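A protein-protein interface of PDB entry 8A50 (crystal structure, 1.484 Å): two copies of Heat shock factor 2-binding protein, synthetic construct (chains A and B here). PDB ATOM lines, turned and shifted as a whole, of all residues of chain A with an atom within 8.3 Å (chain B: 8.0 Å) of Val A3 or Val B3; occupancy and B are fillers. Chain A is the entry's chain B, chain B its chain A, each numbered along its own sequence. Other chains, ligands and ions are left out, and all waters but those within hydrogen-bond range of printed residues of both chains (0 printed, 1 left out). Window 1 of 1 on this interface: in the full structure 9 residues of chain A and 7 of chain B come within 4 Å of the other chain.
O of Glu A1 touches CA of Arg B6, 3.6 Å away. Val A3 touches Lys B4. CB of Lys B7 touches CG2 of Val A3 (3.8 Å). Phe B2 touches Val A5. Val A5 touches Val B5. Arg A6 touches Glu B1 (CA to O, 3.5 Å). Arg A6 touches Phe B2 (CG to CE1, 3.6 Å). CD of Lys A7 touches CG2 of Val B3, 3.95 Å away. Val B3 touches Leu A10 (CB to CD1, 3.7 Å). Val B5 touches Leu A10 (CG2 to CD1, 3.9 Å).
Val B3 touches just these residues of chain A: Val A3 (3.5 Å), Lys A4 (3.7 Å), Val A5 (2.8 Å), Lys A7 (3.95 Å) and Leu A10 (3.7 Å). Of the printed residues of chain B, Lys A7 touches Glu B1 and Val B3. Of the printed residues of chain B, Lys A4 touches Val B3. Of the printed residues of chain A, Val B5 touches Phe A2, Val A3, Val A5 and Leu A10. Of the printed residues of chain B, Glu A1 touches Arg B6 and Lys B7. Lys B8 touches none of the printed residues of chain A. Glu B11 touches none of the printed residues of chain A. The nearest residue of chain A that does not touch Val B3 is Arg A6 (5.0 Å).
Of the 10 printed residues of chain B, 7 touch a printed residue of chain A. Hydrophobic or aromatic side chains of chain B within 4 Å of the printed part of chain A: Phe B2, Val B3 and Val B5. Of the 10 printed residues of chain A, 9 touch a printed residue of chain B.
N of Lys B7 is in hydrogen-bond range of O of Glu A1, 3.0 Å away. The backbone carbonyl oxygen (O) of Glu B1 sits at hydrogen-bond distance from the side-chain amino group (NZ) of Lys A8 (3.4 Å). N of Val B3 lies within hydrogen-bond range of O of Val A5 (2.8 Å). O of Val A3 sits close to O of Val B3, at 3.5 Å. O of Glu B1 sits at hydrogen-bond distance from N of Lys A7 (2.9 Å). O of Val B5 is in hydrogen-bond range of N of Val A3 (2.8 Å).
Phe A2 touches Val B5, and with the chains exchanged Val A5 touches Phe B2. Val A3 touches its own counterpart, Val B3. Leu A10 touches Val B3, but with the chains exchanged Val A3 does not touch Leu B10 (4.2 Å). Leu A10 touches Val B5, but with the chains exchanged Val A5 does not touch Leu B10 (4.4 Å). Positions printed for both chains: 1, 2, 3, 4, 5, 6, 7, 8, 10 and 11.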
ATOM      1  N   GLU A   1      10.857  26.415  -6.257  1.00  0.00           N
ATOM      2  CA  GLU A   1      10.472  26.057  -7.617  1.00  0.00           C
ATOM      3  C   GLU A   1      10.039  24.605  -7.677  1.00  0.00           C
ATOM      4  O   GLU A   1      10.642  23.744  -7.033  1.00  0.00           O
ATOM      5  CB  GLU A   1      11.631  26.264  -8.598  1.00  0.00           C
ATOM      6  CG  GLU A   1      11.309  25.910 -10.044  1.00  0.00           C
ATOM      7  CD  GLU A   1      12.429  26.130 -11.037  1.00  0.00           C
ATOM      8  OE1 GLU A   1      12.183  25.929 -12.247  1.00  0.00           O
ATOM      9  OE2 GLU A   1      13.557  26.468 -10.611  1.00  0.00           O
ATOM     10  N   PHE A   2       9.025  24.348  -8.497  1.00  0.00           N
ATOM     11  CA  PHE A   2       8.481  23.027  -8.730  1.00  0.00           C
ATOM     12  C   PHE A   2       8.552  22.708 -10.222  1.00  0.00           C
ATOM     13  O   PHE A   2       8.501  23.602 -11.065  1.00  0.00           O
ATOM     14  CB  PHE A   2       7.018  22.981  -8.277  1.00  0.00           C
ATOM     15  CG  PHE A   2       6.866  23.121  -6.787  1.00  0.00           C
ATOM     16  CD1 PHE A   2       6.740  24.368  -6.202  1.00  0.00           C
ATOM     17  CD2 PHE A   2       6.883  22.012  -5.968  1.00  0.00           C
ATOM     18  CE1 PHE A   2       6.610  24.495  -4.828  1.00  0.00           C
ATOM     19  CE2 PHE A   2       6.735  22.140  -4.597  1.00  0.00           C
ATOM     20  CZ  PHE A   2       6.630  23.382  -4.033  1.00  0.00           C
ATOM     21  N   VAL A   3       8.717  21.429 -10.533  1.00  0.00           N
ATOM     22  CA  VAL A   3       8.718  20.874 -11.876  1.00  0.00           C
ATOM     23  C   VAL A   3       7.438  20.037 -11.969  1.00  0.00           C
ATOM     24  O   VAL A   3       7.120  19.315 -11.024  1.00  0.00           O
ATOM     25  CB  VAL A   3       9.983  19.995 -12.103  1.00  0.00           C
ATOM     26  CG1 VAL A   3       9.944  19.310 -13.467  1.00  0.00           C
ATOM     27  CG2 VAL A   3      11.247  20.825 -11.952  1.00  0.00           C
ATOM     28  N   LYS A   4       6.705  20.129 -13.084  1.00  0.00           N
ATOM     29  CA  LYS A   4       5.503  19.336 -13.270  1.00  0.00           C
ATOM     30  C   LYS A   4       5.969  18.035 -13.875  1.00  0.00           C
ATOM     31  O   LYS A   4       6.572  18.046 -14.948  1.00  0.00           O
ATOM     32  CB  LYS A   4       4.497  20.030 -14.199  1.00  0.00           C
ATOM     33  CG  LYS A   4       3.887  21.271 -13.587  1.00  0.00           C
ATOM     34  CD  LYS A   4       2.850  21.879 -14.524  1.00  0.00           C
ATOM     35  CE  LYS A   4       2.451  23.282 -14.120  1.00  0.00           C
ATOM     36  NZ  LYS A   4       1.418  23.857 -15.032  1.00  0.00           N
ATOM     37  N   VAL A   5       5.788  16.928 -13.151  1.00  0.00           N
ATOM     38  CA  VAL A   5       6.230  15.625 -13.623  1.00  0.00           C
ATOM     39  C   VAL A   5       5.037  14.757 -13.890  1.00  0.00           C
ATOM     40  O   VAL A   5       4.109  14.711 -13.078  1.00  0.00           O
ATOM     41  CB  VAL A   5       7.145  14.951 -12.590  1.00  0.00           C
ATOM     42  CG1 VAL A   5       7.648  13.611 -13.117  1.00  0.00           C
ATOM     43  CG2 VAL A   5       8.316  15.861 -12.229  1.00  0.00           C
ATOM     44  N   ARG A   6       5.088  13.976 -14.969  1.00  0.00           N
ATOM     45  CA  ARG A   6       4.018  13.050 -15.281  1.00  0.00           C
ATOM     46  C   ARG A   6       3.965  11.986 -14.199  1.00  0.00           C
ATOM     47  O   ARG A   6       5.022  11.482 -13.814  1.00  0.00           O
ATOM     48  CB  ARG A   6       4.253  12.362 -16.624  1.00  0.00           C
ATOM     49  CG  ARG A   6       4.357  13.309 -17.808  1.00  0.00           C
ATOM     50  CD  ARG A   6       4.401  12.584 -19.140  1.00  0.00           C
ATOM     51  NE  ARG A   6       5.533  11.661 -19.257  1.00  0.00           N
ATOM     52  CZ  ARG A   6       5.775  10.893 -20.319  1.00  0.00           C
ATOM     53  NH1 ARG A   6       4.972  10.937 -21.380  1.00  0.00           N
ATOM     54  NH2 ARG A   6       6.824  10.078 -20.331  1.00  0.00           N
ATOM     55  N   LYS A   7       2.779  11.657 -13.676  1.00  0.00           N
ATOM     56  CA  LYS A   7       2.665  10.634 -12.635  1.00  0.00           C
ATOM     57  C   LYS A   7       3.268   9.302 -13.088  1.00  0.00           C
ATOM     58  O   LYS A   7       3.949   8.662 -12.299  1.00  0.00           O
ATOM     59  CB  LYS A   7       1.209  10.439 -12.179  1.00  0.00           C
ATOM     60  CG  LYS A   7       0.994   9.402 -11.075  1.00  0.00           C
ATOM     61  CD  LYS A   7       1.784   9.666  -9.787  1.00  0.00           C
ATOM     62  CE  LYS A   7       1.499   8.685  -8.666  1.00  0.00           C
ATOM     63  NZ  LYS A   7       0.111   8.819  -8.136  1.00  0.00           N
ATOM     64  N   LYS A   8       3.111   8.944 -14.366  1.00  0.00           N
ATOM     65  CA  LYS A   8       3.662   7.684 -14.880  1.00  0.00           C
ATOM     66  C   LYS A   8       5.195   7.682 -14.806  1.00  0.00           C
ATOM     67  O   LYS A   8       5.790   6.627 -14.601  1.00  0.00           O
ATOM     68  CB  LYS A   8       3.189   7.414 -16.315  1.00  0.00           C
ATOM     69  CG  LYS A   8       1.672   7.242 -16.396  1.00  0.00           C
ATOM     70  CD  LYS A   8       0.951   8.130 -17.457  1.00  0.00           C
ATOM     71  CE  LYS A   8       1.133   9.646 -17.361  1.00  0.00           C
ATOM     72  NZ  LYS A   8       0.683  10.232 -16.070  1.00  0.00           N
ATOM     73  N   LEU A  10       6.939   9.327 -12.448  1.00  0.00           N
ATOM     74  CA  LEU A  10       7.238   9.108 -11.028  1.00  0.00           C
ATOM     75  C   LEU A  10       7.007   7.656 -10.635  1.00  0.00           C
ATOM     76  O   LEU A  10       7.691   7.143  -9.745  1.00  0.00           O
ATOM     77  CB  LEU A  10       6.407  10.020 -10.128  1.00  0.00           C
ATOM     78  CG  LEU A  10       6.762  11.499 -10.173  1.00  0.00           C
ATOM     79  CD1 LEU A  10       5.930  12.269  -9.182  1.00  0.00           C
ATOM     80  CD2 LEU A  10       8.254  11.745  -9.922  1.00  0.00           C
ATOM     81  N   GLU A  11       6.020   7.002 -11.227  1.00  0.00           N
ATOM     82  CA  GLU A  11       5.745   5.600 -10.961  1.00  0.00           C
ATOM     83  C   GLU A  11       6.909   4.741 -11.491  1.00  0.00           C
ATOM     84  O   GLU A  11       7.354   3.804 -10.820  1.00  0.00           O
ATOM     85  CB  GLU A  11       4.410   5.169 -11.574  1.00  0.00           C
ATOM     86  CG  GLU A  11       3.246   5.804 -10.835  1.00  0.00           C
ATOM     87  CD  GLU A  11       1.900   5.644 -11.504  1.00  0.00           C
ATOM     88  OE1 GLU A  11       1.857   5.471 -12.743  1.00  0.00           O
ATOM     89  OE2 GLU A  11       0.877   5.732 -10.784  1.00  0.00           O
ATOM     90  N   GLU B   1      -1.950  12.590 -15.577  1.00  0.00           N
ATOM     91  CA  GLU B   1      -1.811  13.332 -14.317  1.00  0.00           C
ATOM     92  C   GLU B   1      -0.398  13.889 -14.178  1.00  0.00           C
ATOM     93  O   GLU B   1       0.559  13.267 -14.632  1.00  0.00           O
ATOM     94  CB  GLU B   1      -2.151  12.428 -13.109  1.00  0.00           C
ATOM     95  CG  GLU B   1      -1.910  13.051 -11.735  1.00  0.00           C
ATOM     96  CD  GLU B   1      -2.178  12.167 -10.529  1.00  0.00           C
ATOM     97  OE1 GLU B   1      -2.480  10.966 -10.716  1.00  0.00           O
ATOM     98  OE2 GLU B   1      -2.067  12.674  -9.389  1.00  0.00           O
ATOM     99  N   PHE B   2      -0.277  15.057 -13.534  1.00  0.00           N
ATOM    100  CA  PHE B   2       1.002  15.715 -13.276  1.00  0.00           C
ATOM    101  C   PHE B   2       1.096  15.933 -11.775  1.00  0.00           C
ATOM    102  O   PHE B   2       0.093  16.232 -11.109  1.00  0.00           O
ATOM    103  CB  PHE B   2       1.104  17.063 -13.991  1.00  0.00           C
ATOM    104  CG  PHE B   2       1.290  16.914 -15.477  1.00  0.00           C
ATOM    105  CD1 PHE B   2       2.539  16.658 -16.011  1.00  0.00           C
ATOM    106  CD2 PHE B   2       0.211  16.991 -16.336  1.00  0.00           C
ATOM    107  CE1 PHE B   2       2.706  16.512 -17.380  1.00  0.00           C
ATOM    108  CE2 PHE B   2       0.381  16.833 -17.703  1.00  0.00           C
ATOM    109  CZ  PHE B   2       1.626  16.596 -18.215  1.00  0.00           C
ATOM    110  N   VAL B   3       2.292  15.772 -11.239  1.00  0.00           N
ATOM    111  CA  VAL B   3       2.588  15.959  -9.836  1.00  0.00           C
ATOM    112  C   VAL B   3       3.657  17.034  -9.758  1.00  0.00           C
ATOM    113  O   VAL B   3       4.625  16.981 -10.514  1.00  0.00           O
ATOM    114  CB  VAL B   3       3.088  14.635  -9.213  1.00  0.00           C
ATOM    115  CG1 VAL B   3       3.586  14.847  -7.788  1.00  0.00           C
ATOM    116  CG2 VAL B   3       1.990  13.579  -9.254  1.00  0.00           C
ATOM    117  N   LYS B   4       3.496  17.993  -8.847  1.00  0.00           N
ATOM    118  CA  LYS B   4       4.503  19.020  -8.639  1.00  0.00           C
ATOM    119  C   LYS B   4       5.603  18.427  -7.773  1.00  0.00           C
ATOM    120  O   LYS B   4       5.326  17.878  -6.706  1.00  0.00           O
ATOM    121  CB  LYS B   4       3.905  20.264  -7.954  1.00  0.00           C
ATOM    122  CG  LYS B   4       3.050  21.080  -8.905  1.00  0.00           C
ATOM    123  CD  LYS B   4       2.611  22.411  -8.303  1.00  0.00           C
ATOM    124  CE  LYS B   4       2.003  23.311  -9.351  1.00  0.00           C
ATOM    125  NZ  LYS B   4       1.651  24.648  -8.795  1.00  0.00           N
ATOM    126  N   VAL B   5       6.834  18.517  -8.233  1.00  0.00           N
ATOM    127  CA  VAL B   5       7.978  18.011  -7.494  1.00  0.00           C
ATOM    128  C   VAL B   5       8.955  19.148  -7.312  1.00  0.00           C
ATOM    129  O   VAL B   5       9.237  19.859  -8.269  1.00  0.00           O
ATOM    130  CB  VAL B   5       8.649  16.858  -8.278  1.00  0.00           C
ATOM    131  CG1 VAL B   5       9.836  16.301  -7.495  1.00  0.00           C
ATOM    132  CG2 VAL B   5       7.644  15.746  -8.585  1.00  0.00           C
ATOM    133  N   ARG B   6       9.512  19.311  -6.107  1.00  0.00           N
ATOM    134  CA  ARG B   6      10.501  20.367  -5.869  1.00  0.00           C
ATOM    135  C   ARG B   6      11.716  20.138  -6.757  1.00  0.00           C
ATOM    136  O   ARG B   6      12.290  19.042  -6.738  1.00  0.00           O
ATOM    137  CB  ARG B   6      10.962  20.368  -4.403  1.00  0.00           C
ATOM    138  CG  ARG B   6      10.040  21.096  -3.437  1.00  0.00           C
ATOM    139  CD  ARG B   6      10.717  21.420  -2.103  1.00  0.00           C
ATOM    140  NE  ARG B   6      11.968  22.169  -2.268  1.00  0.00           N
ATOM    141  CZ  ARG B   6      12.051  23.466  -2.560  1.00  0.00           C
ATOM    142  NH1 ARG B   6      10.949  24.190  -2.728  1.00  0.00           N
ATOM    143  NH2 ARG B   6      13.235  24.045  -2.702  1.00  0.00           N
ATOM    144  N   LYS B   7      12.113  21.151  -7.550  1.00  0.00           N
ATOM    145  CA  LYS B   7      13.270  21.035  -8.437  1.00  0.00           C
ATOM    146  C   LYS B   7      14.528  20.694  -7.642  1.00  0.00           C
ATOM    147  O   LYS B   7      15.293  19.839  -8.069  1.00  0.00           O
ATOM    148  CB  LYS B   7      13.501  22.337  -9.222  1.00  0.00           C
ATOM    149  CG  LYS B   7      14.592  22.201 -10.279  1.00  0.00           C
ATOM    150  CD  LYS B   7      14.603  23.339 -11.285  1.00  0.00           C
ATOM    151  CE  LYS B   7      15.519  23.038 -12.454  1.00  0.00           C
ATOM    152  NZ  LYS B   7      14.861  22.151 -13.458  1.00  0.00           N
ATOM    153  N   LYS B   8      14.735  21.336  -6.480  1.00  0.00           N
ATOM    154  CA  LYS B   8      15.905  21.054  -5.656  1.00  0.00           C
ATOM    155  C   LYS B   8      15.905  19.604  -5.128  1.00  0.00           C
ATOM    156  O   LYS B   8      16.986  19.062  -4.918  1.00  0.00           O
ATOM    157  CB  LYS B   8      16.046  22.072  -4.512  1.00  0.00           C
ATOM    158  CG  LYS B   8      16.330  23.496  -5.000  1.00  0.00           C
ATOM    159  CD  LYS B   8      17.627  24.093  -4.441  1.00  0.00           C
ATOM    160  CE  LYS B   8      17.624  24.355  -2.946  1.00  0.00           C
ATOM    161  NZ  LYS B   8      16.567  25.319  -2.533  1.00  0.00           N
ATOM    162  N   LEU B  10      14.648  16.943  -6.915  1.00  0.00           N
ATOM    163  CA  LEU B  10      15.123  16.185  -8.081  1.00  0.00           C
ATOM    164  C   LEU B  10      16.619  16.399  -8.303  1.00  0.00           C
ATOM    165  O   LEU B  10      17.318  15.470  -8.721  1.00  0.00           O
ATOM    166  CB  LEU B  10      14.358  16.584  -9.331  1.00  0.00           C
ATOM    167  CG  LEU B  10      12.916  16.149  -9.397  1.00  0.00           C
ATOM    168  CD1 LEU B  10      12.197  16.851 -10.531  1.00  0.00           C
ATOM    169  CD2 LEU B  10      12.800  14.636  -9.530  1.00  0.00           C
ATOM    170  N   GLU B  11      17.133  17.624  -8.052  1.00  0.00           N
ATOM    171  CA  GLU B  11      18.551  17.878  -8.196  1.00  0.00           C
ATOM    172  C   GLU B  11      19.334  17.095  -7.132  1.00  0.00           C
ATOM    173  O   GLU B  11      20.393  16.542  -7.443  1.00  0.00           O
ATOM    174  CB  GLU B  11      18.869  19.389  -8.131  1.00  0.00           C
ATOM    175  CG  GLU B  11      18.370  20.138  -9.349  1.00  0.00           C
ATOM    176  CD  GLU B  11      18.513  21.644  -9.269  1.00  0.00           C
ATOM    177  OE1 GLU B  11      18.417  22.188  -8.148  1.00  0.00           O
ATOM    178  OE2 GLU B  11      18.721  22.279 -10.329  1.00  0.00           O
